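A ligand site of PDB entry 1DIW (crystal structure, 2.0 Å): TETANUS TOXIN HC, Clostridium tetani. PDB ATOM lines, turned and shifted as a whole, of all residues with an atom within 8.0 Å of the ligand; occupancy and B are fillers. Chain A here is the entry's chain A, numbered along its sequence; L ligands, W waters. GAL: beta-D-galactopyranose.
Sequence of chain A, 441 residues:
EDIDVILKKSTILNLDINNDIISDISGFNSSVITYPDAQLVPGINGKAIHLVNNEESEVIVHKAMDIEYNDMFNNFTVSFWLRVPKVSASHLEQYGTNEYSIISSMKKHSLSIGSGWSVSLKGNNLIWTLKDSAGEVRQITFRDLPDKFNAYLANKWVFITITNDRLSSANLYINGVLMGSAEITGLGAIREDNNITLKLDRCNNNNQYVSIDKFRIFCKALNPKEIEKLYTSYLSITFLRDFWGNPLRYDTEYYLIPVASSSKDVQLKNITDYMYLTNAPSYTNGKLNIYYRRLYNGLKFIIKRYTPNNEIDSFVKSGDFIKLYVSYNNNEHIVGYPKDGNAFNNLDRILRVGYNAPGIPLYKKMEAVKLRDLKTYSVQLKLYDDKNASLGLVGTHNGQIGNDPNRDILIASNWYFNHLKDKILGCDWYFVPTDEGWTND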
ATOM      1  N   TYR A 250      25.656 -10.780  -3.669  1.00  0.00           N
ATOM      2  CA  TYR A 250      25.388 -11.710  -4.751  1.00  0.00           C
ATOM      3  C   TYR A 250      25.454 -13.129  -4.211  1.00  0.00           C
ATOM      4  O   TYR A 250      26.004 -13.347  -3.154  1.00  0.00           O
ATOM      5  CB  TYR A 250      26.453 -11.573  -5.845  1.00  0.00           C
ATOM      6  CG  TYR A 250      26.126 -10.332  -6.675  1.00  0.00           C
ATOM      7  CD1 TYR A 250      25.027 -10.330  -7.537  1.00  0.00           C
ATOM      8  CD2 TYR A 250      26.891  -9.182  -6.592  1.00  0.00           C
ATOM      9  CE1 TYR A 250      24.690  -9.218  -8.284  1.00  0.00           C
ATOM     10  CE2 TYR A 250      26.568  -8.067  -7.340  1.00  0.00           C
ATOM     11  CZ  TYR A 250      25.468  -8.089  -8.197  1.00  0.00           C
ATOM     12  OH  TYR A 250      25.203  -6.976  -8.953  1.00  0.00           O
ATOM     13  N   ILE A 303      20.364 -13.529  -6.006  1.00  0.00           N
ATOM     14  CA  ILE A 303      20.743 -12.469  -6.913  1.00  0.00           C
ATOM     15  C   ILE A 303      22.049 -12.845  -7.607  1.00  0.00           C
ATOM     16  O   ILE A 303      23.045 -13.196  -6.954  1.00  0.00           O
ATOM     17  CB  ILE A 303      21.020 -11.131  -6.197  1.00  0.00           C
ATOM     18  CG1 ILE A 303      19.852 -10.812  -5.286  1.00  0.00           C
ATOM     19  CG2 ILE A 303      21.266  -9.991  -7.191  1.00  0.00           C
ATOM     20  CD1 ILE A 303      20.169  -9.723  -4.265  1.00  0.00           C
ATOM     21  N   LYS A 304      22.017 -12.857  -8.936  1.00  0.00           N
ATOM     22  CA  LYS A 304      23.248 -13.171  -9.688  1.00  0.00           C
ATOM     23  C   LYS A 304      23.685 -11.989 -10.541  1.00  0.00           C
ATOM     24  O   LYS A 304      22.884 -11.134 -10.968  1.00  0.00           O
ATOM     25  CB  LYS A 304      23.075 -14.427 -10.521  1.00  0.00           C
ATOM     26  CG  LYS A 304      23.059 -15.725  -9.691  1.00  0.00           C
ATOM     27  CD  LYS A 304      23.005 -16.861 -10.718  1.00  0.00           C
ATOM     28  CE  LYS A 304      23.102 -18.229 -10.098  1.00  0.00           C
ATOM     29  NZ  LYS A 304      22.667 -19.293 -11.076  1.00  0.00           N
ATOM     30  N   ARG A 305      25.002 -11.876 -10.729  1.00  0.00           N
ATOM     31  CA  ARG A 305      25.559 -10.788 -11.507  1.00  0.00           C
ATOM     32  C   ARG A 305      25.234 -11.079 -12.971  1.00  0.00           C
ATOM     33  O   ARG A 305      25.254 -12.133 -13.593  1.00  0.00           O
ATOM     34  CB  ARG A 305      26.997 -10.482 -11.205  1.00  0.00           C
ATOM     35  CG  ARG A 305      27.951 -11.573 -11.658  1.00  0.00           C
ATOM     36  CD  ARG A 305      29.305 -11.452 -10.986  1.00  0.00           C
ATOM     37  NE  ARG A 305      29.364 -10.707  -9.757  1.00  0.00           N
ATOM     38  CZ  ARG A 305      29.667 -11.070  -8.558  1.00  0.00           C
ATOM     39  NH1 ARG A 305      30.053 -12.264  -8.129  1.00  0.00           N
ATOM     40  NH2 ARG A 305      29.686 -10.309  -7.496  1.00  0.00           N
ATOM     41  N   TYR A 306      24.678 -10.036 -13.561  1.00  0.00           N
ATOM     42  CA  TYR A 306      24.144 -10.076 -14.914  1.00  0.00           C
ATOM     43  C   TYR A 306      25.248 -10.001 -15.946  1.00  0.00           C
ATOM     44  O   TYR A 306      25.076 -10.411 -17.087  1.00  0.00           O
ATOM     45  CB  TYR A 306      23.190  -8.892 -15.124  1.00  0.00           C
ATOM     46  CG  TYR A 306      22.534  -9.009 -16.469  1.00  0.00           C
ATOM     47  CD1 TYR A 306      21.347  -9.697 -16.620  1.00  0.00           C
ATOM     48  CD2 TYR A 306      23.140  -8.453 -17.585  1.00  0.00           C
ATOM     49  CE1 TYR A 306      20.761  -9.829 -17.864  1.00  0.00           C
ATOM     50  CE2 TYR A 306      22.579  -8.577 -18.841  1.00  0.00           C
ATOM     51  CZ  TYR A 306      21.386  -9.253 -18.956  1.00  0.00           C
ATOM     52  OH  TYR A 306      20.822  -9.361 -20.218  1.00  0.00           O
ATOM     53  N   THR A 307      26.367  -9.488 -15.477  1.00  0.00           N
ATOM     54  CA  THR A 307      27.510  -9.374 -16.380  1.00  0.00           C
ATOM     55  C   THR A 307      28.667  -9.138 -15.425  1.00  0.00           C
ATOM     56  O   THR A 307      28.348  -8.713 -14.319  1.00  0.00           O
ATOM     57  CB  THR A 307      27.291  -8.177 -17.329  1.00  0.00           C
ATOM     58  OG1 THR A 307      27.963  -8.433 -18.564  1.00  0.00           O
ATOM     59  CG2 THR A 307      27.767  -6.844 -16.756  1.00  0.00           C
ATOM     60  N   PRO A 308      29.847  -9.304 -15.966  1.00  0.00           N
ATOM     61  CA  PRO A 308      31.083  -9.056 -15.268  1.00  0.00           C
ATOM     62  C   PRO A 308      31.620  -7.644 -15.452  1.00  0.00           C
ATOM     63  O   PRO A 308      31.655  -6.890 -14.488  1.00  0.00           O
ATOM     64  CB  PRO A 308      32.032 -10.071 -15.940  1.00  0.00           C
ATOM     65  CG  PRO A 308      31.442 -10.485 -17.244  1.00  0.00           C
ATOM     66  CD  PRO A 308      30.109  -9.795 -17.330  1.00  0.00           C
ATOM     67  N   ASN A 309      32.100  -7.309 -16.638  1.00  0.00           N
ATOM     68  CA  ASN A 309      32.698  -6.039 -16.970  1.00  0.00           C
ATOM     69  C   ASN A 309      33.565  -5.493 -15.846  1.00  0.00           C
ATOM     70  O   ASN A 309      33.147  -4.673 -15.023  1.00  0.00           O
ATOM     71  CB  ASN A 309      31.687  -4.976 -17.400  1.00  0.00           C
ATOM     72  CG  ASN A 309      32.349  -4.087 -18.471  1.00  0.00           C
ATOM     73  OD1 ASN A 309      33.010  -3.119 -18.097  1.00  0.00           O
ATOM     74  ND2 ASN A 309      32.172  -4.450 -19.734  1.00  0.00           N
ATOM     75  N   ASN A 310      34.810  -5.965 -15.828  1.00  0.00           N
ATOM     76  CA  ASN A 310      35.808  -5.546 -14.858  1.00  0.00           C
ATOM     77  C   ASN A 310      35.680  -6.051 -13.439  1.00  0.00           C
ATOM     78  O   ASN A 310      35.679  -7.250 -13.148  1.00  0.00           O
ATOM     79  CB  ASN A 310      35.892  -4.021 -14.870  1.00  0.00           C
ATOM     80  CG  ASN A 310      36.796  -3.491 -15.959  1.00  0.00           C
ATOM     81  OD1 ASN A 310      37.186  -2.313 -15.965  1.00  0.00           O
ATOM     82  ND2 ASN A 310      37.181  -4.315 -16.924  1.00  0.00           N
ATOM     83  N   GLU A 311      35.655  -5.120 -12.485  1.00  0.00           N
ATOM     84  CA  GLU A 311      35.669  -5.478 -11.069  1.00  0.00           C
ATOM     85  C   GLU A 311      34.461  -6.300 -10.668  1.00  0.00           C
ATOM     86  O   GLU A 311      33.303  -5.987 -10.914  1.00  0.00           O
ATOM     87  CB  GLU A 311      35.838  -4.206 -10.242  1.00  0.00           C
ATOM     88  CG  GLU A 311      35.284  -4.206  -8.838  1.00  0.00           C
ATOM     89  CD  GLU A 311      34.820  -2.827  -8.398  1.00  0.00           C
ATOM     90  OE1 GLU A 311      34.597  -1.967  -9.286  1.00  0.00           O
ATOM     91  OE2 GLU A 311      34.675  -2.602  -7.179  1.00  0.00           O
ATOM     92  N   ILE A 312      34.747  -7.404  -9.986  1.00  0.00           N
ATOM     93  CA  ILE A 312      33.735  -8.267  -9.413  1.00  0.00           C
ATOM     94  C   ILE A 312      33.579  -7.891  -7.936  1.00  0.00           C
ATOM     95  O   ILE A 312      34.529  -8.010  -7.156  1.00  0.00           O
ATOM     96  CB  ILE A 312      34.129  -9.735  -9.522  1.00  0.00           C
ATOM     97  CG1 ILE A 312      34.087 -10.170 -10.998  1.00  0.00           C
ATOM     98  CG2 ILE A 312      33.203 -10.647  -8.713  1.00  0.00           C
ATOM     99  CD1 ILE A 312      34.853 -11.451 -11.214  1.00  0.00           C
ATOM    100  N   ASP A 313      32.409  -7.442  -7.522  1.00  0.00           N
ATOM    101  CA  ASP A 313      32.201  -7.146  -6.089  1.00  0.00           C
ATOM    102  C   ASP A 313      31.277  -8.175  -5.477  1.00  0.00           C
ATOM    103  O   ASP A 313      30.336  -8.580  -6.160  1.00  0.00           O
ATOM    104  CB  ASP A 313      31.635  -5.748  -5.871  1.00  0.00           C
ATOM    105  CG  ASP A 313      32.590  -4.678  -6.342  1.00  0.00           C
ATOM    106  OD1 ASP A 313      33.814  -4.835  -6.128  1.00  0.00           O
ATOM    107  OD2 ASP A 313      32.123  -3.682  -6.945  1.00  0.00           O
ATOM    108  N   SER A 314      31.409  -8.564  -4.220  1.00  0.00           N
ATOM    109  CA  SER A 314      30.427  -9.472  -3.652  1.00  0.00           C
ATOM    110  C   SER A 314      29.189  -8.705  -3.170  1.00  0.00           C
ATOM    111  O   SER A 314      28.147  -9.311  -2.924  1.00  0.00           O
ATOM    112  CB  SER A 314      31.002 -10.330  -2.530  1.00  0.00           C
ATOM    113  OG  SER A 314      31.305  -9.461  -1.448  1.00  0.00           O
ATOM    114  N   PHE A 315      29.270  -7.384  -3.036  1.00  0.00           N
ATOM    115  CA  PHE A 315      28.100  -6.617  -2.615  1.00  0.00           C
ATOM    116  C   PHE A 315      27.339  -6.118  -3.833  1.00  0.00           C
ATOM    117  O   PHE A 315      27.941  -5.865  -4.879  1.00  0.00           O
ATOM    118  CB  PHE A 315      28.512  -5.441  -1.709  1.00  0.00           C
ATOM    119  CG  PHE A 315      29.146  -6.016  -0.461  1.00  0.00           C
ATOM    120  CD1 PHE A 315      30.437  -5.686  -0.134  1.00  0.00           C
ATOM    121  CD2 PHE A 315      28.473  -6.918   0.348  1.00  0.00           C
ATOM    122  CE1 PHE A 315      31.051  -6.217   0.992  1.00  0.00           C
ATOM    123  CE2 PHE A 315      29.104  -7.433   1.454  1.00  0.00           C
ATOM    124  CZ  PHE A 315      30.381  -7.097   1.806  1.00  0.00           C
ATOM    125  N   VAL A 316      26.042  -5.973  -3.729  1.00  0.00           N
ATOM    126  CA  VAL A 316      25.190  -5.506  -4.808  1.00  0.00           C
ATOM    127  C   VAL A 316      25.048  -3.990  -4.699  1.00  0.00           C
ATOM    128  O   VAL A 316      24.582  -3.542  -3.641  1.00  0.00           O
ATOM    129  CB  VAL A 316      23.779  -6.093  -4.695  1.00  0.00           C
ATOM    130  CG1 VAL A 316      22.946  -5.694  -5.898  1.00  0.00           C
ATOM    131  CG2 VAL A 316      23.866  -7.617  -4.518  1.00  0.00           C
ATOM    132  N   LYS A 317      25.398  -3.258  -5.737  1.00  0.00           N
ATOM    133  CA  LYS A 317      25.281  -1.803  -5.740  1.00  0.00           C
ATOM    134  C   LYS A 317      23.979  -1.366  -6.372  1.00  0.00           C
ATOM    135  O   LYS A 317      23.438  -2.028  -7.257  1.00  0.00           O
ATOM    136  CB  LYS A 317      26.449  -1.166  -6.494  1.00  0.00           C
ATOM    137  CG  LYS A 317      27.798  -1.361  -5.818  1.00  0.00           C
ATOM    138  CD  LYS A 317      28.899  -0.651  -6.587  1.00  0.00           C
ATOM    139  CE  LYS A 317      29.240  -1.391  -7.888  1.00  0.00           C
ATOM    140  NZ  LYS A 317      30.224  -2.474  -7.668  1.00  0.00           N
ATOM    141  N   GLY A 319      21.632   0.137  -8.926  1.00  0.00           N
ATOM    142  CA  GLY A 319      21.878   0.326 -10.336  1.00  0.00           C
ATOM    143  C   GLY A 319      22.541  -0.873 -10.995  1.00  0.00           C
ATOM    144  O   GLY A 319      22.680  -0.897 -12.216  1.00  0.00           O
ATOM    145  N   ASP A 320      22.997  -1.851 -10.221  1.00  0.00           N
ATOM    146  CA  ASP A 320      23.601  -3.049 -10.789  1.00  0.00           C
ATOM    147  C   ASP A 320      22.534  -3.765 -11.596  1.00  0.00           C
ATOM    148  O   ASP A 320      21.405  -3.751 -11.090  1.00  0.00           O
ATOM    149  CB  ASP A 320      24.027  -3.990  -9.658  1.00  0.00           C
ATOM    150  CG  ASP A 320      25.408  -3.733  -9.111  1.00  0.00           C
ATOM    151  OD1 ASP A 320      25.988  -2.719  -9.526  1.00  0.00           O
ATOM    152  OD2 ASP A 320      25.890  -4.541  -8.287  1.00  0.00           O
ATOM    153  N   PHE A 321      22.828  -4.380 -12.705  1.00  0.00           N
ATOM    154  CA  PHE A 321      21.888  -5.202 -13.473  1.00  0.00           C
ATOM    155  C   PHE A 321      22.074  -6.605 -12.935  1.00  0.00           C
ATOM    156  O   PHE A 321      23.188  -7.075 -12.744  1.00  0.00           O
ATOM    157  CB  PHE A 321      22.133  -5.154 -14.990  1.00  0.00           C
ATOM    158  CG  PHE A 321      21.676  -3.789 -15.491  1.00  0.00           C
ATOM    159  CD1 PHE A 321      20.350  -3.570 -15.728  1.00  0.00           C
ATOM    160  CD2 PHE A 321      22.587  -2.763 -15.645  1.00  0.00           C
ATOM    161  CE1 PHE A 321      19.867  -2.324 -16.141  1.00  0.00           C
ATOM    162  CE2 PHE A 321      22.127  -1.522 -16.052  1.00  0.00           C
ATOM    163  CZ  PHE A 321      20.778  -1.298 -16.295  1.00  0.00           C
ATOM    164  N   ILE A 322      21.009  -7.317 -12.619  1.00  0.00           N
ATOM    165  CA  ILE A 322      21.004  -8.604 -11.985  1.00  0.00           C
ATOM    166  C   ILE A 322      20.009  -9.539 -12.649  1.00  0.00           C
ATOM    167  O   ILE A 322      19.219  -9.103 -13.495  1.00  0.00           O
ATOM    168  CB  ILE A 322      20.670  -8.477 -10.485  1.00  0.00           C
ATOM    169  CG1 ILE A 322      19.253  -7.917 -10.239  1.00  0.00           C
ATOM    170  CG2 ILE A 322      21.607  -7.596  -9.691  1.00  0.00           C
ATOM    171  CD1 ILE A 322      18.233  -8.927  -9.785  1.00  0.00           C
ATOM    172  N   LYS A 323      20.080 -10.810 -12.292  1.00  0.00           N
ATOM    173  CA  LYS A 323      19.176 -11.865 -12.676  1.00  0.00           C
ATOM    174  C   LYS A 323      18.714 -12.469 -11.342  1.00  0.00           C
ATOM    175  O   LYS A 323      19.544 -12.633 -10.454  1.00  0.00           O
ATOM    176  CB  LYS A 323      19.743 -12.973 -13.570  1.00  0.00           C
ATOM    177  CG  LYS A 323      19.968 -12.485 -14.995  1.00  0.00           C
ATOM    178  CD  LYS A 323      21.159 -13.175 -15.681  1.00  0.00           C
ATOM    179  CE  LYS A 323      20.711 -14.400 -16.438  1.00  0.00           C
ATOM    180  NZ  LYS A 323      21.638 -14.816 -17.539  1.00  0.00           N
ATOM    181  N   LYS A 365      16.218  -9.430 -17.430  1.00  0.00           N
ATOM    182  CA  LYS A 365      17.199  -8.494 -16.941  1.00  0.00           C
ATOM    183  C   LYS A 365      16.466  -7.529 -15.967  1.00  0.00           C
ATOM    184  O   LYS A 365      15.475  -6.876 -16.305  1.00  0.00           O
ATOM    185  CB  LYS A 365      17.892  -7.730 -18.047  1.00  0.00           C
ATOM    186  CG  LYS A 365      18.682  -6.503 -17.636  1.00  0.00           C
ATOM    187  CD  LYS A 365      19.500  -5.985 -18.820  1.00  0.00           C
ATOM    188  CE  LYS A 365      19.689  -4.488 -18.792  1.00  0.00           C
ATOM    189  NZ  LYS A 365      20.505  -3.940 -19.927  1.00  0.00           N
ATOM    190  N   MET A 366      17.042  -7.468 -14.770  1.00  0.00           N
ATOM    191  CA  MET A 366      16.515  -6.605 -13.745  1.00  0.00           C
ATOM    192  C   MET A 366      17.604  -5.649 -13.307  1.00  0.00           C
ATOM    193  O   MET A 366      18.758  -5.911 -13.599  1.00  0.00           O
ATOM    194  CB  MET A 366      16.054  -7.344 -12.487  1.00  0.00           C
ATOM    195  CG  MET A 366      14.740  -8.097 -12.678  1.00  0.00           C
ATOM    196  SD  MET A 366      14.198  -8.774 -11.082  1.00  0.00           S
ATOM    197  CE  MET A 366      12.996  -9.953 -11.707  1.00  0.00           C
ATOM    198  N   GLU A 367      17.202  -4.610 -12.618  1.00  0.00           N
ATOM    199  CA  GLU A 367      18.118  -3.626 -12.077  1.00  0.00           C
ATOM    200  C   GLU A 367      17.769  -3.462 -10.586  1.00  0.00           C
ATOM    201  O   GLU A 367      16.591  -3.242 -10.322  1.00  0.00           O
ATOM    202  CB  GLU A 367      17.985  -2.310 -12.830  1.00  0.00           C
ATOM    203  CG  GLU A 367      19.036  -1.271 -12.449  1.00  0.00           C
ATOM    204  CD  GLU A 367      18.745   0.103 -13.032  1.00  0.00           C
ATOM    205  OE1 GLU A 367      17.714   0.254 -13.741  1.00  0.00           O
ATOM    206  OE2 GLU A 367      19.536   1.033 -12.758  1.00  0.00           O
HETATM  207  C1  GAL L   1      27.803  -4.401 -12.540  1.00  0.00           C
HETATM  208  C2  GAL L   1      26.807  -5.437 -13.031  1.00  0.00           C
HETATM  209  C3  GAL L   1      26.463  -6.416 -11.932  1.00  0.00           C
HETATM  210  C4  GAL L   1      27.732  -6.914 -11.238  1.00  0.00           C
HETATM  211  C5  GAL L   1      28.549  -5.736 -10.708  1.00  0.00           C
HETATM  212  C6  GAL L   1      29.786  -6.207  -9.972  1.00  0.00           C
HETATM  213  O1  GAL L   1      28.251  -3.775 -13.720  1.00  0.00           O
HETATM  214  O2  GAL L   1      25.700  -4.755 -13.659  1.00  0.00           O
HETATM  215  O3  GAL L   1      25.669  -7.491 -12.440  1.00  0.00           O
HETATM  216  O4  GAL L   1      28.582  -7.616 -12.141  1.00  0.00           O
HETATM  217  O5  GAL L   1      28.921  -4.950 -11.870  1.00  0.00           O
HETATM  218  O6  GAL L   1      29.781  -7.588  -9.590  1.00  0.00           O
HETATM  219  O   HOH W   1      28.446  -4.538  -7.316  1.00  0.00           O
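O of Thr 307 lies within hydrogen-bond range of O4 of the ligand (2.4 Å). N of Phe 321 lies within hydrogen-bond range of O2 of the ligand. The backbone carbonyl oxygen (O) of Phe 321 lies within hydrogen-bond range of an oxygen (O3) of the ligand, at 2.5 Å. N of Tyr 306 sits at hydrogen-bond distance from O3 of the ligand (3.0 Å). An oxygen (O6) of the ligand is in hydrogen-bond range of the guanidinium group (NE) of Arg 305. An oxygen (O6) of the ligand lies within hydrogen-bond range of the backbone NH (N) of Asp 313, at 3.3 Å.
O of Phe 321 lies close to N of Tyr 306, 3.4 Å away. OD2 of Asp 320 lies within hydrogen-bond range of OH of Tyr 250. The backbone NH (N) of Tyr 250 sits at hydrogen-bond distance from the backbone carbonyl oxygen (O) of Ser 314 (3.0 Å). OD1 of Asp 313 sits close to OE2 of Glu 311. OD2 of Asp 320 lies within hydrogen-bond range of N of Lys 317 (2.9 Å).
Tyr 250 touches the ligand. Pro 308 touches the ligand. Glu 311 touches the ligand (O to C6, 3.6 Å). Asp 320 touches the ligand (OD2 to C5, 3.8 Å). Hydrophobic or aromatic side chains within 4 Å of the ligand: Tyr 250, Tyr 306 and Phe 321. Within 4 Å of the ligand: Tyr 250, Arg 305, Tyr 306, Thr 307, Pro 308, Glu 311, Asp 313, Asp 320 and Phe 321.
Water W1 lies within hydrogen-bond range of the side-chain carboxylate (OD2) of Asp 320 (2.7 Å), the side-chain amino group (NZ) of Lys 317 (2.7 Å) and the backbone carbonyl oxygen (O) of Phe 315 (2.8 Å).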
